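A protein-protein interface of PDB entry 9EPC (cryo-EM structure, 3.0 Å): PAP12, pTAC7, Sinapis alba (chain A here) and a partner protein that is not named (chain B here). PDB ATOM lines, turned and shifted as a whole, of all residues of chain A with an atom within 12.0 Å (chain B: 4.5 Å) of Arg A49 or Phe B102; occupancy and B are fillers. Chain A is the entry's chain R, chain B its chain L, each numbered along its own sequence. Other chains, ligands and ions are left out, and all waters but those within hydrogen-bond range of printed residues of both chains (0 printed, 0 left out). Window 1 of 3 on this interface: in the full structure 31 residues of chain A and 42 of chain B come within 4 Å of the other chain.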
ATOM      1  N   GLY A  35     -12.738  -7.466 -12.020  1.00  0.00           N
ATOM      2  CA  GLY A  35     -12.593  -6.744 -10.770  1.00  0.00           C
ATOM      3  C   GLY A  35     -12.702  -5.242 -10.929  1.00  0.00           C
ATOM      4  O   GLY A  35     -13.794  -4.682 -10.849  1.00  0.00           O
ATOM      5  N   ARG A  44     -14.464   5.084 -11.317  1.00  0.00           N
ATOM      6  CA  ARG A  44     -14.667   3.660 -11.093  1.00  0.00           C
ATOM      7  C   ARG A  44     -16.157   3.353 -11.035  1.00  0.00           C
ATOM      8  O   ARG A  44     -16.916   4.052 -10.357  1.00  0.00           O
ATOM      9  CB  ARG A  44     -13.985   3.207  -9.799  1.00  0.00           C
ATOM     10  CG  ARG A  44     -12.468   3.341  -9.800  1.00  0.00           C
ATOM     11  CD  ARG A  44     -11.821   2.462  -8.734  1.00  0.00           C
ATOM     12  NE  ARG A  44     -12.135   1.052  -8.935  1.00  0.00           N
ATOM     13  CZ  ARG A  44     -11.718   0.068  -8.151  1.00  0.00           C
ATOM     14  NH1 ARG A  44     -10.941   0.297  -7.104  1.00  0.00           N
ATOM     15  NH2 ARG A  44     -12.093  -1.179  -8.422  1.00  0.00           N
ATOM     16  N   ILE A  45     -16.571   2.311 -11.751  1.00  0.00           N
ATOM     17  CA  ILE A  45     -17.960   1.868 -11.779  1.00  0.00           C
ATOM     18  C   ILE A  45     -18.038   0.493 -11.137  1.00  0.00           C
ATOM     19  O   ILE A  45     -17.297  -0.424 -11.514  1.00  0.00           O
ATOM     20  CB  ILE A  45     -18.523   1.852 -13.210  1.00  0.00           C
ATOM     21  CG1 ILE A  45     -17.485   1.308 -14.195  1.00  0.00           C
ATOM     22  CG2 ILE A  45     -18.978   3.245 -13.613  1.00  0.00           C
ATOM     23  CD1 ILE A  45     -17.855  -0.033 -14.776  1.00  0.00           C
ATOM     24  N   TRP A  46     -18.923   0.356 -10.158  1.00  0.00           N
ATOM     25  CA  TRP A  46     -19.052  -0.860  -9.377  1.00  0.00           C
ATOM     26  C   TRP A  46     -20.508  -1.291  -9.357  1.00  0.00           C
ATOM     27  O   TRP A  46     -21.420  -0.465  -9.459  1.00  0.00           O
ATOM     28  CB  TRP A  46     -18.534  -0.659  -7.945  1.00  0.00           C
ATOM     29  CG  TRP A  46     -18.774   0.722  -7.405  1.00  0.00           C
ATOM     30  CD1 TRP A  46     -18.124   1.867  -7.765  1.00  0.00           C
ATOM     31  CD2 TRP A  46     -19.721   1.101  -6.397  1.00  0.00           C
ATOM     32  NE1 TRP A  46     -18.613   2.933  -7.055  1.00  0.00           N
ATOM     33  CE2 TRP A  46     -19.592   2.491  -6.208  1.00  0.00           C
ATOM     34  CE3 TRP A  46     -20.665   0.402  -5.640  1.00  0.00           C
ATOM     35  CZ2 TRP A  46     -20.370   3.194  -5.293  1.00  0.00           C
ATOM     36  CZ3 TRP A  46     -21.436   1.104  -4.732  1.00  0.00           C
ATOM     37  CH2 TRP A  46     -21.285   2.485  -4.569  1.00  0.00           C
ATOM     38  N   ARG A  47     -20.718  -2.597  -9.233  1.00  0.00           N
ATOM     39  CA  ARG A  47     -22.064  -3.152  -9.212  1.00  0.00           C
ATOM     40  C   ARG A  47     -22.716  -2.852  -7.869  1.00  0.00           C
ATOM     41  O   ARG A  47     -22.194  -3.238  -6.818  1.00  0.00           O
ATOM     42  CB  ARG A  47     -22.029  -4.656  -9.469  1.00  0.00           C
ATOM     43  CG  ARG A  47     -23.402  -5.303  -9.483  1.00  0.00           C
ATOM     44  CD  ARG A  47     -23.320  -6.805  -9.689  1.00  0.00           C
ATOM     45  NE  ARG A  47     -22.620  -7.473  -8.598  1.00  0.00           N
ATOM     46  CZ  ARG A  47     -23.202  -7.907  -7.488  1.00  0.00           C
ATOM     47  NH1 ARG A  47     -24.500  -7.753  -7.282  1.00  0.00           N
ATOM     48  NH2 ARG A  47     -22.463  -8.511  -6.562  1.00  0.00           N
ATOM     49  N   ARG A  48     -23.857  -2.169  -7.903  1.00  0.00           N
ATOM     50  CA  ARG A  48     -24.571  -1.816  -6.681  1.00  0.00           C
ATOM     51  C   ARG A  48     -25.280  -3.052  -6.146  1.00  0.00           C
ATOM     52  O   ARG A  48     -26.319  -3.457  -6.676  1.00  0.00           O
ATOM     53  CB  ARG A  48     -25.563  -0.692  -6.960  1.00  0.00           C
ATOM     54  CG  ARG A  48     -25.028   0.379  -7.891  1.00  0.00           C
ATOM     55  CD  ARG A  48     -23.787   1.035  -7.318  1.00  0.00           C
ATOM     56  NE  ARG A  48     -23.027   1.756  -8.332  1.00  0.00           N
ATOM     57  CZ  ARG A  48     -23.185   3.042  -8.613  1.00  0.00           C
ATOM     58  NH1 ARG A  48     -24.071   3.787  -7.975  1.00  0.00           N
ATOM     59  NH2 ARG A  48     -22.433   3.595  -9.561  1.00  0.00           N
ATOM     60  N   ARG A  49     -24.722  -3.656  -5.101  1.00  0.00           N
ATOM     61  CA  ARG A  49     -25.294  -4.875  -4.545  1.00  0.00           C
ATOM     62  C   ARG A  49     -26.650  -4.575  -3.918  1.00  0.00           C
ATOM     63  O   ARG A  49     -26.749  -3.778  -2.979  1.00  0.00           O
ATOM     64  CB  ARG A  49     -24.340  -5.486  -3.523  1.00  0.00           C
ATOM     65  CG  ARG A  49     -23.242  -6.325  -4.157  1.00  0.00           C
ATOM     66  CD  ARG A  49     -22.258  -6.854  -3.131  1.00  0.00           C
ATOM     67  NE  ARG A  49     -21.265  -5.855  -2.755  1.00  0.00           N
ATOM     68  CZ  ARG A  49     -20.220  -6.097  -1.975  1.00  0.00           C
ATOM     69  NH1 ARG A  49     -20.008  -7.297  -1.460  1.00  0.00           N
ATOM     70  NH2 ARG A  49     -19.368  -5.113  -1.708  1.00  0.00           N
ATOM     71  N   THR A  50     -27.692  -5.212  -4.445  1.00  0.00           N
ATOM     72  CA  THR A  50     -29.063  -4.971  -4.029  1.00  0.00           C
ATOM     73  C   THR A  50     -29.754  -6.307  -3.798  1.00  0.00           C
ATOM     74  O   THR A  50     -29.396  -7.320  -4.405  1.00  0.00           O
ATOM     75  CB  THR A  50     -29.827  -4.148  -5.084  1.00  0.00           C
ATOM     76  OG1 THR A  50     -29.038  -3.016  -5.471  1.00  0.00           O
ATOM     77  CG2 THR A  50     -31.159  -3.652  -4.537  1.00  0.00           C
ATOM     78  N   LEU A  51     -30.747  -6.300  -2.913  1.00  0.00           N
ATOM     79  CA  LEU A  51     -31.494  -7.508  -2.571  1.00  0.00           C
ATOM     80  C   LEU A  51     -32.274  -7.966  -3.796  1.00  0.00           C
ATOM     81  O   LEU A  51     -33.286  -7.368  -4.166  1.00  0.00           O
ATOM     82  CB  LEU A  51     -32.423  -7.235  -1.394  1.00  0.00           C
ATOM     83  CG  LEU A  51     -33.216  -8.425  -0.858  1.00  0.00           C
ATOM     84  CD1 LEU A  51     -32.280  -9.496  -0.327  1.00  0.00           C
ATOM     85  CD2 LEU A  51     -34.182  -7.968   0.220  1.00  0.00           C
ATOM     86  N   THR A  52     -31.800  -9.038  -4.434  1.00  0.00           N
ATOM     87  CA  THR A  52     -32.436  -9.514  -5.658  1.00  0.00           C
ATOM     88  C   THR A  52     -33.819 -10.082  -5.374  1.00  0.00           C
ATOM     89  O   THR A  52     -34.796  -9.733  -6.048  1.00  0.00           O
ATOM     90  CB  THR A  52     -31.556 -10.569  -6.328  1.00  0.00           C
ATOM     91  OG1 THR A  52     -31.779 -11.840  -5.706  1.00  0.00           O
ATOM     92  CG2 THR A  52     -30.089 -10.200  -6.184  1.00  0.00           C
ATOM     93  N   LYS A  53     -33.922 -10.956  -4.379  1.00  0.00           N
ATOM     94  CA  LYS A  53     -35.186 -11.589  -4.034  1.00  0.00           C
ATOM     95  C   LYS A  53     -35.987 -10.656  -3.126  1.00  0.00           C
ATOM     96  O   LYS A  53     -35.593  -9.517  -2.861  1.00  0.00           O
ATOM     97  CB  LYS A  53     -34.930 -12.953  -3.401  1.00  0.00           C
ATOM     98  CG  LYS A  53     -33.839 -12.944  -2.348  1.00  0.00           C
ATOM     99  CD  LYS A  53     -33.325 -14.345  -2.076  1.00  0.00           C
ATOM    100  CE  LYS A  53     -32.702 -14.947  -3.324  1.00  0.00           C
ATOM    101  NZ  LYS A  53     -32.143 -16.303  -3.075  1.00  0.00           N
ATOM    102  N   LEU A  58     -40.205  -7.974   5.540  1.00  0.00           N
ATOM    103  CA  LEU A  58     -39.879  -6.563   5.366  1.00  0.00           C
ATOM    104  C   LEU A  58     -41.133  -5.699   5.347  1.00  0.00           C
ATOM    105  O   LEU A  58     -41.170  -4.632   5.971  1.00  0.00           O
ATOM    106  CB  LEU A  58     -39.074  -6.371   4.083  1.00  0.00           C
ATOM    107  CG  LEU A  58     -37.691  -5.754   4.273  1.00  0.00           C
ATOM    108  CD1 LEU A  58     -36.979  -5.606   2.941  1.00  0.00           C
ATOM    109  CD2 LEU A  58     -37.818  -4.415   4.969  1.00  0.00           C
ATOM    110  N   ALA B  75     -25.475   2.477   1.343  1.00  0.00           N
ATOM    111  CA  ALA B  75     -25.868   1.136   0.949  1.00  0.00           C
ATOM    112  C   ALA B  75     -27.373   1.069   0.705  1.00  0.00           C
ATOM    113  O   ALA B  75     -28.133   1.979   1.048  1.00  0.00           O
ATOM    114  CB  ALA B  75     -25.459   0.122   2.015  1.00  0.00           C
ATOM    115  N   ASP B  76     -27.794  -0.028   0.090  1.00  0.00           N
ATOM    116  CA  ASP B  76     -29.211  -0.266  -0.132  1.00  0.00           C
ATOM    117  C   ASP B  76     -29.938  -0.276   1.208  1.00  0.00           C
ATOM    118  O   ASP B  76     -29.518  -0.993   2.126  1.00  0.00           O
ATOM    119  CB  ASP B  76     -29.407  -1.596  -0.858  1.00  0.00           C
ATOM    120  CG  ASP B  76     -30.861  -1.895  -1.161  1.00  0.00           C
ATOM    121  OD1 ASP B  76     -31.665  -0.947  -1.254  1.00  0.00           O
ATOM    122  OD2 ASP B  76     -31.200  -3.087  -1.305  1.00  0.00           O
ATOM    123  N   PHE B  79     -30.568  -3.514   2.880  1.00  0.00           N
ATOM    124  CA  PHE B  79     -29.463  -4.236   3.507  1.00  0.00           C
ATOM    125  C   PHE B  79     -29.567  -4.188   5.024  1.00  0.00           C
ATOM    126  O   PHE B  79     -29.466  -5.218   5.699  1.00  0.00           O
ATOM    127  CB  PHE B  79     -28.127  -3.660   3.043  1.00  0.00           C
ATOM    128  CG  PHE B  79     -26.939  -4.231   3.759  1.00  0.00           C
ATOM    129  CD1 PHE B  79     -26.474  -5.497   3.456  1.00  0.00           C
ATOM    130  CD2 PHE B  79     -26.283  -3.499   4.731  1.00  0.00           C
ATOM    131  CE1 PHE B  79     -25.381  -6.025   4.111  1.00  0.00           C
ATOM    132  CE2 PHE B  79     -25.189  -4.021   5.389  1.00  0.00           C
ATOM    133  CZ  PHE B  79     -24.739  -5.286   5.078  1.00  0.00           C
ATOM    134  N   LYS B  96     -21.882   2.012   4.109  1.00  0.00           N
ATOM    135  CA  LYS B  96     -21.602   2.634   2.826  1.00  0.00           C
ATOM    136  C   LYS B  96     -20.843   1.654   1.945  1.00  0.00           C
ATOM    137  O   LYS B  96     -20.044   0.846   2.430  1.00  0.00           O
ATOM    138  CB  LYS B  96     -20.794   3.922   2.989  1.00  0.00           C
ATOM    139  CG  LYS B  96     -21.503   5.002   3.781  1.00  0.00           C
ATOM    140  CD  LYS B  96     -20.655   6.255   3.873  1.00  0.00           C
ATOM    141  CE  LYS B  96     -21.377   7.352   4.633  1.00  0.00           C
ATOM    142  NZ  LYS B  96     -20.559   8.591   4.732  1.00  0.00           N
ATOM    143  N   GLU B  97     -21.101   1.732   0.646  1.00  0.00           N
ATOM    144  CA  GLU B  97     -20.476   0.853  -0.327  1.00  0.00           C
ATOM    145  C   GLU B  97     -19.763   1.678  -1.387  1.00  0.00           C
ATOM    146  O   GLU B  97     -20.110   2.837  -1.636  1.00  0.00           O
ATOM    147  CB  GLU B  97     -21.508  -0.067  -0.985  1.00  0.00           C
ATOM    148  CG  GLU B  97     -22.728   0.660  -1.521  1.00  0.00           C
ATOM    149  CD  GLU B  97     -23.712  -0.273  -2.193  1.00  0.00           C
ATOM    150  OE1 GLU B  97     -23.332  -1.425  -2.491  1.00  0.00           O
ATOM    151  OE2 GLU B  97     -24.867   0.143  -2.421  1.00  0.00           O
ATOM    152  N   GLY B 101     -15.673  -1.988  -1.880  1.00  0.00           N
ATOM    153  CA  GLY B 101     -16.617  -2.890  -1.257  1.00  0.00           C
ATOM    154  C   GLY B 101     -17.486  -2.142  -0.266  1.00  0.00           C
ATOM    155  O   GLY B 101     -17.671  -0.935  -0.374  1.00  0.00           O
ATOM    156  N   PHE B 102     -18.009  -2.888   0.702  1.00  0.00           N
ATOM    157  CA  PHE B 102     -18.863  -2.317   1.734  1.00  0.00           C
ATOM    158  C   PHE B 102     -18.005  -1.638   2.798  1.00  0.00           C
ATOM    159  O   PHE B 102     -16.800  -1.432   2.628  1.00  0.00           O
ATOM    160  CB  PHE B 102     -19.761  -3.391   2.339  1.00  0.00           C
ATOM    161  CG  PHE B 102     -21.121  -3.468   1.712  1.00  0.00           C
ATOM    162  CD1 PHE B 102     -22.160  -2.686   2.186  1.00  0.00           C
ATOM    163  CD2 PHE B 102     -21.364  -4.323   0.655  1.00  0.00           C
ATOM    164  CE1 PHE B 102     -23.413  -2.755   1.615  1.00  0.00           C
ATOM    165  CE2 PHE B 102     -22.615  -4.395   0.078  1.00  0.00           C
ATOM    166  CZ  PHE B 102     -23.641  -3.610   0.561  1.00  0.00           C
ATOM    167  N   GLY B 103     -18.627  -1.285   3.916  1.00  0.00           N
ATOM    168  CA  GLY B 103     -17.924  -0.634   5.000  1.00  0.00           C
ATOM    169  C   GLY B 103     -18.868   0.089   5.934  1.00  0.00           C
ATOM    170  O   GLY B 103     -19.932   0.552   5.515  1.00  0.00           O
ATOM    171  N   ASP B 186     -27.050 -12.180  -1.061  1.00  0.00           N
ATOM    172  CA  ASP B 186     -27.090 -11.283  -2.207  1.00  0.00           C
ATOM    173  C   ASP B 186     -26.138 -10.107  -2.052  1.00  0.00           C
ATOM    174  O   ASP B 186     -25.705  -9.540  -3.059  1.00  0.00           O
ATOM    175  CB  ASP B 186     -28.513 -10.773  -2.433  1.00  0.00           C
ATOM    176  CG  ASP B 186     -29.467 -11.875  -2.841  1.00  0.00           C
ATOM    177  OD1 ASP B 186     -29.030 -13.041  -2.920  1.00  0.00           O
ATOM    178  OD2 ASP B 186     -30.655 -11.575  -3.085  1.00  0.00           O
ATOM    179  N   PHE B 187     -25.804  -9.730  -0.822  1.00  0.00           N
ATOM    180  CA  PHE B 187     -24.871  -8.643  -0.574  1.00  0.00           C
ATOM    181  C   PHE B 187     -23.429  -9.114  -0.474  1.00  0.00           C
ATOM    182  O   PHE B 187     -22.531  -8.285  -0.297  1.00  0.00           O
ATOM    183  CB  PHE B 187     -25.263  -7.894   0.700  1.00  0.00           C
ATOM    184  CG  PHE B 187     -26.614  -7.254   0.625  1.00  0.00           C
ATOM    185  CD1 PHE B 187     -26.767  -5.996   0.071  1.00  0.00           C
ATOM    186  CD2 PHE B 187     -27.733  -7.910   1.101  1.00  0.00           C
ATOM    187  CE1 PHE B 187     -28.011  -5.405  -0.002  1.00  0.00           C
ATOM    188  CE2 PHE B 187     -28.979  -7.323   1.030  1.00  0.00           C
ATOM    189  CZ  PHE B 187     -29.117  -6.069   0.477  1.00  0.00           C
ATOM    190  N   LEU B 188     -23.185 -10.417  -0.571  1.00  0.00           N
ATOM    191  CA  LEU B 188     -21.823 -10.908  -0.642  1.00  0.00           C
ATOM    192  C   LEU B 188     -21.227 -10.585  -2.011  1.00  0.00           C
ATOM    193  O   LEU B 188     -21.947 -10.527  -3.011  1.00  0.00           O
ATOM    194  CB  LEU B 188     -21.780 -12.412  -0.402  1.00  0.00           C
ATOM    195  CG  LEU B 188     -22.329 -12.900   0.937  1.00  0.00           C
ATOM    196  CD1 LEU B 188     -22.201 -14.407   1.031  1.00  0.00           C
ATOM    197  CD2 LEU B 188     -21.607 -12.227   2.086  1.00  0.00           C
ATOM    198  N   PRO B 189     -19.919 -10.357  -2.082  1.00  0.00           N
ATOM    199  CA  PRO B 189     -19.293 -10.115  -3.383  1.00  0.00           C
ATOM    200  C   PRO B 189     -19.346 -11.358  -4.254  1.00  0.00           C
ATOM    201  O   PRO B 189     -19.292 -12.490  -3.771  1.00  0.00           O
ATOM    202  CB  PRO B 189     -17.849  -9.750  -3.020  1.00  0.00           C
ATOM    203  CG  PRO B 189     -17.619 -10.431  -1.719  1.00  0.00           C
ATOM    204  CD  PRO B 189     -18.931 -10.376  -0.991  1.00  0.00           C
ATOM    205  N   GLU B 193     -15.944 -10.057  -7.880  1.00  0.00           N
ATOM    206  CA  GLU B 193     -15.786  -8.979  -6.912  1.00  0.00           C
ATOM    207  C   GLU B 193     -14.980  -9.393  -5.689  1.00  0.00           C
ATOM    208  O   GLU B 193     -14.349  -8.534  -5.063  1.00  0.00           O
ATOM    209  CB  GLU B 193     -17.157  -8.464  -6.473  1.00  0.00           C
ATOM    210  CG  GLU B 193     -18.011  -7.941  -7.613  1.00  0.00           C
ATOM    211  CD  GLU B 193     -19.412  -7.577  -7.171  1.00  0.00           C
ATOM    212  OE1 GLU B 193     -19.672  -7.586  -5.950  1.00  0.00           O
ATOM    213  OE2 GLU B 193     -20.254  -7.285  -8.045  1.00  0.00           O
ATOM    214  N   MET B 284     -18.487  -7.114   7.479  1.00  0.00           N
ATOM    215  CA  MET B 284     -18.365  -5.898   6.684  1.00  0.00           C
ATOM    216  C   MET B 284     -17.365  -4.917   7.283  1.00  0.00           C
ATOM    217  O   MET B 284     -16.895  -4.021   6.575  1.00  0.00           O
ATOM    218  CB  MET B 284     -19.729  -5.224   6.532  1.00  0.00           C
ATOM    219  CG  MET B 284     -20.818  -6.092   5.916  1.00  0.00           C
ATOM    220  SD  MET B 284     -20.548  -6.499   4.181  1.00  0.00           S
ATOM    221  CE  MET B 284     -19.878  -8.153   4.321  1.00  0.00           C
ATOM    222  N   ASN B 286     -13.962  -3.465   8.124  1.00  0.00           N
ATOM    223  CA  ASN B 286     -12.665  -3.636   7.495  1.00  0.00           C
ATOM    224  C   ASN B 286     -11.583  -3.852   8.549  1.00  0.00           C
ATOM    225  O   ASN B 286     -11.807  -3.711   9.753  1.00  0.00           O
ATOM    226  CB  ASN B 286     -12.333  -2.435   6.615  1.00  0.00           C
ATOM    227  CG  ASN B 286     -13.107  -2.442   5.315  1.00  0.00           C
ATOM    228  OD1 ASN B 286     -13.465  -3.501   4.801  1.00  0.00           O
ATOM    229  ND2 ASN B 286     -13.369  -1.260   4.775  1.00  0.00           N
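O of Trp A46 is in hydrogen-bond range of NE of Arg A48, at 3.0 Å. OG1 of Thr A50 is in hydrogen-bond range of O of Arg A48, 3.0 Å away.
Printed residues of chain A that touch a printed residue of chain B: Trp A46, Arg A47, Arg A49, Thr A50, Leu A51, Thr A52 and Lys A53. Hydrophobic or aromatic side chains of chain A that line the printed part of chain B: Trp A46 and Leu A51. Of the 15 printed residues of chain B, 9 touch a printed residue of chain A. Printed residues of chain B that touch a printed residue of chain A: Asp B76, Glu B97, Gly B101, Phe B102, Asp B186, Phe B187, Leu B188, Pro B189 and Glu B193. Hydrophobic or aromatic side chains of chain B that line the printed part of chain A: Phe B102, Phe B187 and Pro B189. Among the printed residues, Asp or Glu carboxylates within 4 Å of a Lys or Arg side-chain nitrogen of the other chain: Arg A47 with Glu B193 (2.4 Å) and Arg A49 with Glu B193 (3.97 Å).
Arg A49 touches seven residues of chain B. Of chain A, only Arg A49 comes within 4 Å of Phe B102. No residue of chain A comes within 4 Å of Ala B75. Printed residues of chain A within 4 Å of Asp B76: Thr A50 (3.3 Å) and Leu A51 (3.6 Å). Phe B79 touches none of the printed residues of chain A. Glu B97 touches just these residues of chain A: Trp A46 and Arg A49. Of chain A, only Arg A49 (3.6 Å) comes within 4 Å of Gly B101. No residue of chain A comes within 4 Å of Gly B103. Phe B187 touches two residues of chain A. Of chain A, only Arg A49 (3.5 Å) comes within 4 Å of Leu B188. Of the printed residues of chain A, Pro B189 touches Arg A49. No residue of chain A comes within 4 Å of Met B284. Of the printed residues of chain A, Asp B186 touches Leu A51 (3.8 Å), Thr A52 (2.9 Å) and Lys A53 (3.5 Å). Of the printed residues of chain B, Leu A51 touches Asp B76 (3.6 Å), Asp B186 (3.8 Å) and Phe B187 (3.8 Å). Printed residues of chain B within 4 Å of Trp A46: Glu B97. Printed residues of chain B within 4 Å of Thr A52: Asp B186. Lys B96 touches none of the printed residues of chain A. Asn B286 touches none of the printed residues of chain A. The nearest residue of chain B that does not touch Arg A49 is Asp B76 (4.04 Å).
The side-chain carboxylate (OD2) of Asp B186 is in hydrogen-bond range of the side-chain hydroxyl (OG1) of Thr A52, 2.9 Å away. O of Phe B187 is in hydrogen-bond range of NH1 of Arg A49 (2.9 Å). The guanidinium group (NE) of Arg A47 lies within salt-bridge range of the side-chain carboxylate (OE2) of Glu B193 (2.4 Å). The side-chain carboxylate of Glu B193 is in salt-bridge range of the guanidinium group of Arg A49, 3.97 Å away. The guanidinium group (NH1) of Arg A49 lies close to the backbone nitrogen (N) of Pro B189.
Among the printed residues, pairs that only touch across the chains: Trp A46 with Glu B97, Arg A49 with Phe B102, Thr A50 with Asp B76, Lys A53 with Asp B186, Arg A49 with Leu B188, Arg A49 with Gly B101, Leu A51 with Asp B76, Arg A49 with Glu B97, Leu A51 with Phe B187 and Leu A51 with Asp B186.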
